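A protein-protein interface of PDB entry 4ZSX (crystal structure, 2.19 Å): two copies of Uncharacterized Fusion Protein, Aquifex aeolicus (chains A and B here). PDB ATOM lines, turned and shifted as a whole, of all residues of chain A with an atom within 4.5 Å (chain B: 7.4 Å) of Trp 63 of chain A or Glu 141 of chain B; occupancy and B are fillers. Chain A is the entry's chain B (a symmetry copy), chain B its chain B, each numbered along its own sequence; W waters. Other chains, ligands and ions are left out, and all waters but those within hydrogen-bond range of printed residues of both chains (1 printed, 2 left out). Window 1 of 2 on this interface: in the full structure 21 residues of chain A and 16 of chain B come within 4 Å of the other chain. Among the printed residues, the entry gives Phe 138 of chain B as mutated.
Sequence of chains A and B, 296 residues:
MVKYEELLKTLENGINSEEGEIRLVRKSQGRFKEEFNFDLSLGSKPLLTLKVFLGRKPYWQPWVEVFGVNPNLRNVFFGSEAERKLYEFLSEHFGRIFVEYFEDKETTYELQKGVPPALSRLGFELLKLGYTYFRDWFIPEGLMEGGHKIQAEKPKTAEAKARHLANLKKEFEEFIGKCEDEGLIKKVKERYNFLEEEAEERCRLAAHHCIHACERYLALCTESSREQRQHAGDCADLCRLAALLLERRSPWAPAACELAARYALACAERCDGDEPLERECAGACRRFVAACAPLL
OE1 of Glu 65 of chain A sits close to O of Gly 142 of chain B, 3.5 Å away.
The side-chain carboxylate of Glu 145 of chain B lies close to the side-chain carboxylate of Glu 35 of chain A, 2.6 Å away.
OE1 of Glu 145 of chain B lies within salt-bridge range of NZ of Lys 51 of chain A, at 3.7 Å.
N of Phe 53 of chain A sits at hydrogen-bond distance from O of Trp 63 of chain A, 3.0 Å away.
The side-chain carboxylate of Glu 141 of chain B sits at hydrogen-bond distance from the backbone NH of Gly 146 of chain B, 2.7 Å away.
The backbone carbonyl oxygen of Val 64 of chain A sits at hydrogen-bond distance from the backbone NH of Phe 98 of chain A (3.0 Å).
N of Lys 51 of chain A lies within hydrogen-bond range of O of Glu 65 of chain A (2.6 Å).
The side-chain carboxylate of Glu 141 of chain B is in hydrogen-bond range of a ring nitrogen (ND1) of His 148 of chain B (2.5 Å).
The side-chain carboxylate (OE1) of Glu 141 of chain B lies within hydrogen-bond range of the backbone NH (N) of Gly 147 of chain B, 3.4 Å away.
Phe 32 of chain A touches Glu 100 of chain B.
Phe 32 of chain A touches Phe 102 of chain B (CD1 to CD2, 3.1 Å).
OE2 of Glu 141 of chain B touches CE2 of Phe 32 of chain A (3.9 Å).
Phe 53 of chain A touches Phe 102 of chain B (CZ to CE1, 3.4 Å).
Glu 141 of chain B touches Trp 63 of chain A (CB to CZ2, 3.6 Å).
Trp 63 of chain A touches Gly 142 of chain B.
Arg 96 of chain A touches Pro 140 of chain B (NH1 to CB, 3.7 Å).
CB of Pro 140 of chain B touches CZ of Phe 98 of chain A (3.7 Å).
CE1 of Phe 98 of chain A touches CA of Gly 142 of chain B (3.5 Å).
Phe 98 of chain A touches Leu 143 of chain B (CE2 to N, 3.7 Å).
Gln 61 of chain A touches none of the printed residues of chain B.
Trp 63 of chain A touches just these residues of chain B: Glu 141 (3.6 Å) and Gly 142 (3.8 Å).
Printed residues of chain B within 4 Å of Glu 65 of chain A: Gly 142 (3.5 Å).
Of the printed residues of chain A, Glu 100 of chain B touches Phe 32.
Glu 141 of chain B touches two residues of chain A.
The nearest printed residue of chain B that does not touch Glu 35 of chain A is Glu 141 of chain B (5.3 Å).
Of the 13 printed residues of chain A, 8 touch a printed residue of chain B.
Hydrophobic or aromatic side chains of chain A within 4 Å of the printed part of chain B: Phe 32, Phe 53, Trp 63 and Phe 98.
Printed residues of chain B that touch a printed residue of chain A: Glu 100, Phe 102, Pro 140, Glu 141, Gly 142, Leu 143 and Glu 145.
Hydrophobic or aromatic side chains of chain B that line the printed part of chain A: Phe 102 and Pro 140.
Among the printed residues, Asp or Glu carboxylates within 4 Å of a Lys or Arg side-chain nitrogen of the other chain: Lys 51 of chain A with Glu 145 of chain B.
No position is printed for both chains.
Of the 13 pairs that touch across the chains among the printed residues, none has its exchanged pair printed and touching as well.
Water W1 bridges the backbone NH (N) of Glu 141 of chain B (2.8 Å) and the guanidinium group (NH1) of Arg 96 of chain A (2.9 Å).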
ATOM      1  N   PHE A  32      18.816  19.493 -16.562  1.00  0.00           N
ATOM      2  CA  PHE A  32      18.209  20.666 -15.954  1.00  0.00           C
ATOM      3  C   PHE A  32      18.333  20.522 -14.462  1.00  0.00           C
ATOM      4  O   PHE A  32      18.656  19.439 -13.983  1.00  0.00           O
ATOM      5  CB  PHE A  32      16.750  20.803 -16.372  1.00  0.00           C
ATOM      6  CG  PHE A  32      16.578  21.115 -17.826  1.00  0.00           C
ATOM      7  CD1 PHE A  32      16.621  22.430 -18.268  1.00  0.00           C
ATOM      8  CD2 PHE A  32      16.409  20.097 -18.767  1.00  0.00           C
ATOM      9  CE1 PHE A  32      16.471  22.746 -19.622  1.00  0.00           C
ATOM     10  CE2 PHE A  32      16.271  20.396 -20.134  1.00  0.00           C
ATOM     11  CZ  PHE A  32      16.300  21.732 -20.558  1.00  0.00           C
ATOM     12  N   GLU A  35      16.459  17.903 -12.843  1.00  0.00           N
ATOM     13  CA  GLU A  35      16.728  16.638 -13.522  1.00  0.00           C
ATOM     14  C   GLU A  35      17.884  15.799 -12.947  1.00  0.00           C
ATOM     15  O   GLU A  35      18.926  16.345 -12.618  1.00  0.00           O
ATOM     16  CB  GLU A  35      16.987  16.917 -14.987  1.00  0.00           C
ATOM     17  CG  GLU A  35      16.849  15.702 -15.837  1.00  0.00           C
ATOM     18  CD  GLU A  35      17.227  15.972 -17.256  1.00  0.00           C
ATOM     19  OE1 GLU A  35      16.378  16.524 -17.984  1.00  0.00           O
ATOM     20  OE2 GLU A  35      18.383  15.653 -17.627  1.00  0.00           O
ATOM     21  N   LYS A  51      16.383   8.141 -15.356  1.00  0.00           N
ATOM     22  CA  LYS A  51      16.603   9.575 -15.535  1.00  0.00           C
ATOM     23  C   LYS A  51      15.351  10.297 -15.098  1.00  0.00           C
ATOM     24  O   LYS A  51      14.280  10.019 -15.617  1.00  0.00           O
ATOM     25  CB  LYS A  51      16.949   9.912 -16.975  1.00  0.00           C
ATOM     26  CG  LYS A  51      17.318  11.352 -17.181  1.00  0.00           C
ATOM     27  CD  LYS A  51      17.490  11.652 -18.656  1.00  0.00           C
ATOM     28  CE  LYS A  51      18.755  11.043 -19.238  1.00  0.00           C
ATOM     29  NZ  LYS A  51      19.982  11.724 -18.739  1.00  0.00           N
ATOM     30  N   VAL A  52      15.447  11.198 -14.129  1.00  0.00           N
ATOM     31  CA  VAL A  52      14.220  11.802 -13.638  1.00  0.00           C
ATOM     32  C   VAL A  52      14.167  13.309 -13.775  1.00  0.00           C
ATOM     33  O   VAL A  52      15.153  13.992 -13.608  1.00  0.00           O
ATOM     34  CB  VAL A  52      13.966  11.459 -12.171  1.00  0.00           C
ATOM     35  CG1 VAL A  52      14.354  10.028 -11.907  1.00  0.00           C
ATOM     36  CG2 VAL A  52      14.716  12.377 -11.265  1.00  0.00           C
ATOM     37  N   PHE A  53      12.984  13.810 -14.111  1.00  0.00           N
ATOM     38  CA  PHE A  53      12.695  15.228 -14.082  1.00  0.00           C
ATOM     39  C   PHE A  53      11.584  15.365 -13.073  1.00  0.00           C
ATOM     40  O   PHE A  53      10.611  14.636 -13.135  1.00  0.00           O
ATOM     41  CB  PHE A  53      12.279  15.750 -15.453  1.00  0.00           C
ATOM     42  CG  PHE A  53      11.818  17.184 -15.452  1.00  0.00           C
ATOM     43  CD1 PHE A  53      12.691  18.205 -15.171  1.00  0.00           C
ATOM     44  CD2 PHE A  53      10.507  17.506 -15.742  1.00  0.00           C
ATOM     45  CE1 PHE A  53      12.265  19.510 -15.179  1.00  0.00           C
ATOM     46  CE2 PHE A  53      10.086  18.811 -15.751  1.00  0.00           C
ATOM     47  CZ  PHE A  53      10.965  19.811 -15.468  1.00  0.00           C
ATOM     48  N   GLN A  61       5.474  18.857 -16.438  1.00  0.00           N
ATOM     49  CA  GLN A  61       5.232  17.657 -15.654  1.00  0.00           C
ATOM     50  C   GLN A  61       6.500  16.868 -15.384  1.00  0.00           C
ATOM     51  O   GLN A  61       7.447  16.906 -16.161  1.00  0.00           O
ATOM     52  CB  GLN A  61       4.213  16.752 -16.354  1.00  0.00           C
ATOM     53  CG  GLN A  61       2.828  17.340 -16.493  1.00  0.00           C
ATOM     54  CD  GLN A  61       2.266  17.832 -15.169  1.00  0.00           C
ATOM     55  OE1 GLN A  61       2.266  17.110 -14.165  1.00  0.00           O
ATOM     56  NE2 GLN A  61       1.794  19.068 -15.156  1.00  0.00           N
ATOM     57  N   PRO A  62       6.513  16.148 -14.258  1.00  0.00           N
ATOM     58  CA  PRO A  62       7.560  15.189 -13.947  1.00  0.00           C
ATOM     59  C   PRO A  62       7.506  14.046 -14.933  1.00  0.00           C
ATOM     60  O   PRO A  62       6.449  13.783 -15.489  1.00  0.00           O
ATOM     61  CB  PRO A  62       7.196  14.709 -12.540  1.00  0.00           C
ATOM     62  CG  PRO A  62       6.259  15.692 -12.016  1.00  0.00           C
ATOM     63  CD  PRO A  62       5.523  16.226 -13.177  1.00  0.00           C
ATOM     64  N   TRP A  63       8.631  13.399 -15.173  1.00  0.00           N
ATOM     65  CA  TRP A  63       8.636  12.199 -15.966  1.00  0.00           C
ATOM     66  C   TRP A  63       9.832  11.413 -15.514  1.00  0.00           C
ATOM     67  O   TRP A  63      10.701  11.956 -14.865  1.00  0.00           O
ATOM     68  CB  TRP A  63       8.662  12.522 -17.464  1.00  0.00           C
ATOM     69  CG  TRP A  63       9.751  13.461 -17.898  1.00  0.00           C
ATOM     70  CD1 TRP A  63       9.636  14.790 -18.135  1.00  0.00           C
ATOM     71  CD2 TRP A  63      11.113  13.123 -18.161  1.00  0.00           C
ATOM     72  NE1 TRP A  63      10.840  15.306 -18.519  1.00  0.00           N
ATOM     73  CE2 TRP A  63      11.765  14.300 -18.542  1.00  0.00           C
ATOM     74  CE3 TRP A  63      11.846  11.930 -18.105  1.00  0.00           C
ATOM     75  CZ2 TRP A  63      13.109  14.329 -18.858  1.00  0.00           C
ATOM     76  CZ3 TRP A  63      13.167  11.956 -18.417  1.00  0.00           C
ATOM     77  CH2 TRP A  63      13.794  13.147 -18.790  1.00  0.00           C
ATOM     78  N   VAL A  64       9.870  10.132 -15.829  1.00  0.00           N
ATOM     79  CA  VAL A  64      11.008   9.328 -15.466  1.00  0.00           C
ATOM     80  C   VAL A  64      11.375   8.458 -16.631  1.00  0.00           C
ATOM     81  O   VAL A  64      10.516   7.989 -17.345  1.00  0.00           O
ATOM     82  CB  VAL A  64      10.714   8.464 -14.243  1.00  0.00           C
ATOM     83  CG1 VAL A  64       9.570   7.503 -14.512  1.00  0.00           C
ATOM     84  CG2 VAL A  64      11.931   7.712 -13.830  1.00  0.00           C
ATOM     85  N   GLU A  65      12.659   8.263 -16.858  1.00  0.00           N
ATOM     86  CA  GLU A  65      13.069   7.392 -17.934  1.00  0.00           C
ATOM     87  C   GLU A  65      13.909   6.231 -17.404  1.00  0.00           C
ATOM     88  O   GLU A  65      14.898   6.418 -16.713  1.00  0.00           O
ATOM     89  CB  GLU A  65      13.842   8.189 -18.979  1.00  0.00           C
ATOM     90  CG  GLU A  65      14.487   7.361 -20.042  1.00  0.00           C
ATOM     91  CD  GLU A  65      15.566   8.106 -20.773  1.00  0.00           C
ATOM     92  OE1 GLU A  65      15.718   9.324 -20.549  1.00  0.00           O
ATOM     93  OE2 GLU A  65      16.273   7.479 -21.581  1.00  0.00           O
ATOM     94  N   PHE A  94       5.187   9.549 -10.622  1.00  0.00           N
ATOM     95  CA  PHE A  94       5.337  10.012 -12.010  1.00  0.00           C
ATOM     96  C   PHE A  94       4.175   9.730 -12.921  1.00  0.00           C
ATOM     97  O   PHE A  94       3.775   8.589 -13.056  1.00  0.00           O
ATOM     98  CB  PHE A  94       6.553   9.376 -12.645  1.00  0.00           C
ATOM     99  CG  PHE A  94       7.818   9.809 -12.040  1.00  0.00           C
ATOM    100  CD1 PHE A  94       8.388  11.004 -12.401  1.00  0.00           C
ATOM    101  CD2 PHE A  94       8.431   9.045 -11.081  1.00  0.00           C
ATOM    102  CE1 PHE A  94       9.562  11.417 -11.833  1.00  0.00           C
ATOM    103  CE2 PHE A  94       9.596   9.451 -10.519  1.00  0.00           C
ATOM    104  CZ  PHE A  94      10.165  10.641 -10.892  1.00  0.00           C
ATOM    105  N   ARG A  96       4.257  10.344 -16.237  1.00  0.00           N
ATOM    106  CA  ARG A  96       4.759  10.027 -17.554  1.00  0.00           C
ATOM    107  C   ARG A  96       5.964   9.190 -17.339  1.00  0.00           C
ATOM    108  O   ARG A  96       6.767   9.504 -16.490  1.00  0.00           O
ATOM    109  CB  ARG A  96       5.119  11.277 -18.348  1.00  0.00           C
ATOM    110  CG  ARG A  96       5.619  10.960 -19.757  1.00  0.00           C
ATOM    111  CD  ARG A  96       6.257  12.152 -20.501  1.00  0.00           C
ATOM    112  NE  ARG A  96       5.308  12.961 -21.273  1.00  0.00           N
ATOM    113  CZ  ARG A  96       5.653  13.916 -22.140  1.00  0.00           C
ATOM    114  NH1 ARG A  96       6.924  14.189 -22.402  1.00  0.00           N
ATOM    115  NH2 ARG A  96       4.715  14.592 -22.771  1.00  0.00           N
ATOM    116  N   PHE A  98       9.035   6.595 -19.499  1.00  0.00           N
ATOM    117  CA  PHE A  98       9.646   6.058 -20.721  1.00  0.00           C
ATOM    118  C   PHE A  98      10.436   4.807 -20.377  1.00  0.00           C
ATOM    119  O   PHE A  98      11.144   4.794 -19.391  1.00  0.00           O
ATOM    120  CB  PHE A  98      10.602   7.046 -21.383  1.00  0.00           C
ATOM    121  CG  PHE A  98       9.999   8.366 -21.743  1.00  0.00           C
ATOM    122  CD1 PHE A  98       9.750   9.314 -20.783  1.00  0.00           C
ATOM    123  CD2 PHE A  98       9.743   8.676 -23.061  1.00  0.00           C
ATOM    124  CE1 PHE A  98       9.231  10.521 -21.117  1.00  0.00           C
ATOM    125  CE2 PHE A  98       9.218   9.884 -23.398  1.00  0.00           C
ATOM    126  CZ  PHE A  98       8.963  10.807 -22.424  1.00  0.00           C
ATOM    127  N   GLU B 100      16.345  27.050 -26.775  1.00  0.00           N
ATOM    128  CA  GLU B 100      15.675  26.217 -25.782  1.00  0.00           C
ATOM    129  C   GLU B 100      14.706  27.011 -24.923  1.00  0.00           C
ATOM    130  O   GLU B 100      15.133  27.941 -24.263  1.00  0.00           O
ATOM    131  CB  GLU B 100      16.711  25.592 -24.863  1.00  0.00           C
ATOM    132  CG  GLU B 100      17.088  24.190 -25.169  1.00  0.00           C
ATOM    133  CD  GLU B 100      17.893  23.573 -24.051  1.00  0.00           C
ATOM    134  OE1 GLU B 100      18.361  24.313 -23.161  1.00  0.00           O
ATOM    135  OE2 GLU B 100      18.061  22.344 -24.068  1.00  0.00           O
ATOM    136  N   PHE B 102      12.637  25.851 -22.093  1.00  0.00           N
ATOM    137  CA  PHE B 102      12.204  25.316 -20.785  1.00  0.00           C
ATOM    138  C   PHE B 102      12.165  26.410 -19.720  1.00  0.00           C
ATOM    139  O   PHE B 102      11.210  26.501 -18.954  1.00  0.00           O
ATOM    140  CB  PHE B 102      13.107  24.138 -20.314  1.00  0.00           C
ATOM    141  CG  PHE B 102      12.940  23.756 -18.833  1.00  0.00           C
ATOM    142  CD1 PHE B 102      11.790  23.124 -18.367  1.00  0.00           C
ATOM    143  CD2 PHE B 102      13.939  24.020 -17.913  1.00  0.00           C
ATOM    144  CE1 PHE B 102      11.643  22.782 -17.009  1.00  0.00           C
ATOM    145  CE2 PHE B 102      13.798  23.671 -16.568  1.00  0.00           C
ATOM    146  CZ  PHE B 102      12.646  23.058 -16.122  1.00  0.00           C
ATOM    147  N   TRP B 137       9.687  22.889 -31.970  1.00  0.00           N
ATOM    148  CA  TRP B 137      10.051  21.547 -31.579  1.00  0.00           C
ATOM    149  C   TRP B 137       9.626  21.301 -30.173  1.00  0.00           C
ATOM    150  O   TRP B 137       9.818  22.157 -29.334  1.00  0.00           O
ATOM    151  CB  TRP B 137      11.547  21.350 -31.690  1.00  0.00           C
ATOM    152  CG  TRP B 137      12.045  21.524 -33.054  1.00  0.00           C
ATOM    153  CD1 TRP B 137      12.608  22.639 -33.596  1.00  0.00           C
ATOM    154  CD2 TRP B 137      12.026  20.546 -34.078  1.00  0.00           C
ATOM    155  NE1 TRP B 137      12.947  22.410 -34.902  1.00  0.00           N
ATOM    156  CE2 TRP B 137      12.601  21.126 -35.220  1.00  0.00           C
ATOM    157  CE3 TRP B 137      11.586  19.224 -34.140  1.00  0.00           C
ATOM    158  CZ2 TRP B 137      12.743  20.436 -36.401  1.00  0.00           C
ATOM    159  CZ3 TRP B 137      11.726  18.545 -35.310  1.00  0.00           C
ATOM    160  CH2 TRP B 137      12.298  19.146 -36.429  1.00  0.00           C
ATOM    161  N   PHE B 138       9.037  20.144 -29.905  1.00  0.00           N
ATOM    162  CA  PHE B 138       8.742  19.774 -28.530  1.00  0.00           C
ATOM    163  C   PHE B 138       8.780  18.271 -28.370  1.00  0.00           C
ATOM    164  O   PHE B 138       7.880  17.671 -27.812  1.00  0.00           O
ATOM    165  CB  PHE B 138       7.402  20.333 -28.089  1.00  0.00           C
ATOM    166  CG  PHE B 138       6.295  20.069 -29.045  1.00  0.00           C
ATOM    167  CD1 PHE B 138       6.154  20.828 -30.190  1.00  0.00           C
ATOM    168  CD2 PHE B 138       5.363  19.083 -28.779  1.00  0.00           C
ATOM    169  CE1 PHE B 138       5.128  20.581 -31.073  1.00  0.00           C
ATOM    170  CE2 PHE B 138       4.329  18.832 -29.649  1.00  0.00           C
ATOM    171  CZ  PHE B 138       4.207  19.581 -30.797  1.00  0.00           C
ATOM    172  N   ILE B 139       9.862  17.685 -28.856  1.00  0.00           N
ATOM    173  CA  ILE B 139      10.182  16.289 -28.642  1.00  0.00           C
ATOM    174  C   ILE B 139      10.347  15.957 -27.174  1.00  0.00           C
ATOM    175  O   ILE B 139      11.060  16.655 -26.457  1.00  0.00           O
ATOM    176  CB  ILE B 139      11.446  15.963 -29.362  1.00  0.00           C
ATOM    177  CG1 ILE B 139      11.267  16.339 -30.814  1.00  0.00           C
ATOM    178  CG2 ILE B 139      11.803  14.511 -29.191  1.00  0.00           C
ATOM    179  CD1 ILE B 139      12.534  16.481 -31.526  1.00  0.00           C
ATOM    180  N   PRO B 140       9.691  14.883 -26.718  1.00  0.00           N
ATOM    181  CA  PRO B 140       9.769  14.494 -25.306  1.00  0.00           C
ATOM    182  C   PRO B 140      11.202  14.306 -24.840  1.00  0.00           C
ATOM    183  O   PRO B 140      11.927  13.533 -25.463  1.00  0.00           O
ATOM    184  CB  PRO B 140       9.010  13.173 -25.262  1.00  0.00           C
ATOM    185  CG  PRO B 140       8.237  13.097 -26.515  1.00  0.00           C
ATOM    186  CD  PRO B 140       8.826  13.997 -27.511  1.00  0.00           C
ATOM    187  N   GLU B 141      11.589  14.956 -23.744  1.00  0.00           N
ATOM    188  CA  GLU B 141      12.975  14.899 -23.306  1.00  0.00           C
ATOM    189  C   GLU B 141      13.310  13.491 -22.888  1.00  0.00           C
ATOM    190  O   GLU B 141      14.457  13.076 -22.958  1.00  0.00           O
ATOM    191  CB  GLU B 141      13.242  15.862 -22.157  1.00  0.00           C
ATOM    192  CG  GLU B 141      12.850  17.320 -22.415  1.00  0.00           C
ATOM    193  CD  GLU B 141      13.876  18.160 -23.177  1.00  0.00           C
ATOM    194  OE1 GLU B 141      13.460  19.076 -23.915  1.00  0.00           O
ATOM    195  OE2 GLU B 141      15.094  17.958 -23.000  1.00  0.00           O
ATOM    196  N   GLY B 142      12.299  12.737 -22.485  1.00  0.00           N
ATOM    197  CA  GLY B 142      12.495  11.342 -22.138  1.00  0.00           C
ATOM    198  C   GLY B 142      12.920  10.516 -23.333  1.00  0.00           C
ATOM    199  O   GLY B 142      13.509   9.457 -23.197  1.00  0.00           O
ATOM    200  N   LEU B 143      12.609  11.003 -24.523  1.00  0.00           N
ATOM    201  CA  LEU B 143      12.961  10.283 -25.724  1.00  0.00           C
ATOM    202  C   LEU B 143      14.280  10.833 -26.201  1.00  0.00           C
ATOM    203  O   LEU B 143      15.216  10.098 -26.486  1.00  0.00           O
ATOM    204  CB  LEU B 143      11.865  10.440 -26.768  1.00  0.00           C
ATOM    205  CG  LEU B 143      12.013   9.831 -28.153  1.00  0.00           C
ATOM    206  CD1 LEU B 143      12.809  10.739 -29.007  1.00  0.00           C
ATOM    207  CD2 LEU B 143      12.647   8.465 -28.103  1.00  0.00           C
ATOM    208  N   MET B 144      14.341  12.152 -26.262  1.00  0.00           N
ATOM    209  CA  MET B 144      15.539  12.839 -26.656  1.00  0.00           C
ATOM    210  C   MET B 144      15.582  14.178 -25.962  1.00  0.00           C
ATOM    211  O   MET B 144      14.629  14.938 -26.024  1.00  0.00           O
ATOM    212  CB  MET B 144      15.555  13.025 -28.158  1.00  0.00           C
ATOM    213  CG  MET B 144      16.689  13.857 -28.672  1.00  0.00           C
ATOM    214  SD  MET B 144      16.243  14.605 -30.240  1.00  0.00           S
ATOM    215  CE  MET B 144      15.737  16.228 -29.732  1.00  0.00           C
ATOM    216  N   GLU B 145      16.679  14.467 -25.279  1.00  0.00           N
ATOM    217  CA  GLU B 145      16.823  15.737 -24.576  1.00  0.00           C
ATOM    218  C   GLU B 145      17.207  16.862 -25.506  1.00  0.00           C
ATOM    219  O   GLU B 145      17.892  16.653 -26.498  1.00  0.00           O
ATOM    220  CB  GLU B 145      17.840  15.646 -23.446  1.00  0.00           C
ATOM    221  CG  GLU B 145      17.384  14.743 -22.318  1.00  0.00           C
ATOM    222  CD  GLU B 145      18.223  14.876 -21.076  1.00  0.00           C
ATOM    223  OE1 GLU B 145      19.416  14.500 -21.050  1.00  0.00           O
ATOM    224  OE2 GLU B 145      17.656  15.388 -20.101  1.00  0.00           O
ATOM    225  N   GLY B 146      16.748  18.062 -25.190  1.00  0.00           N
ATOM    226  CA  GLY B 146      17.126  19.217 -25.967  1.00  0.00           C
ATOM    227  C   GLY B 146      16.215  19.306 -27.156  1.00  0.00           C
ATOM    228  O   GLY B 146      16.600  19.735 -28.223  1.00  0.00           O
ATOM    229  N   GLY B 147      14.984  18.874 -26.968  1.00  0.00           N
ATOM    230  CA  GLY B 147      14.060  18.824 -28.067  1.00  0.00           C
ATOM    231  C   GLY B 147      12.980  19.853 -27.892  1.00  0.00           C
ATOM    232  O   GLY B 147      12.013  19.861 -28.627  1.00  0.00           O
ATOM    233  N   HIS B 148      13.141  20.746 -26.933  1.00  0.00           N
ATOM    234  CA  HIS B 148      12.174  21.811 -26.798  1.00  0.00           C
ATOM    235  C   HIS B 148      12.765  23.132 -27.208  1.00  0.00           C
ATOM    236  O   HIS B 148      13.253  23.895 -26.392  1.00  0.00           O
ATOM    237  CB  HIS B 148      11.653  21.859 -25.379  1.00  0.00           C
ATOM    238  CG  HIS B 148      10.707  20.745 -25.072  1.00  0.00           C
ATOM    239  ND1 HIS B 148      11.134  19.494 -24.692  1.00  0.00           N
ATOM    240  CD2 HIS B 148       9.360  20.676 -25.149  1.00  0.00           C
ATOM    241  CE1 HIS B 148      10.087  18.709 -24.520  1.00  0.00           C
ATOM    242  NE2 HIS B 148       9.000  19.403 -24.792  1.00  0.00           N
ATOM    243  N   LYS B 149      12.663  23.412 -28.495  1.00  0.00           N
ATOM    244  CA  LYS B 149      13.378  24.501 -29.099  1.00  0.00           C
ATOM    245  C   LYS B 149      12.522  25.167 -30.121  1.00  0.00           C
ATOM    246  O   LYS B 149      11.711  24.515 -30.747  1.00  0.00           O
ATOM    247  CB  LYS B 149      14.648  24.000 -29.760  1.00  0.00           C
ATOM    248  CG  LYS B 149      15.710  23.624 -28.791  1.00  0.00           C
ATOM    249  CD  LYS B 149      16.760  22.832 -29.463  1.00  0.00           C
ATOM    250  CE  LYS B 149      17.829  22.473 -28.496  1.00  0.00           C
ATOM    251  NZ  LYS B 149      18.779  21.534 -29.146  1.00  0.00           N
HETATM  252  O   HOH W   1       9.259  15.877 -22.485  1.00  0.00           O
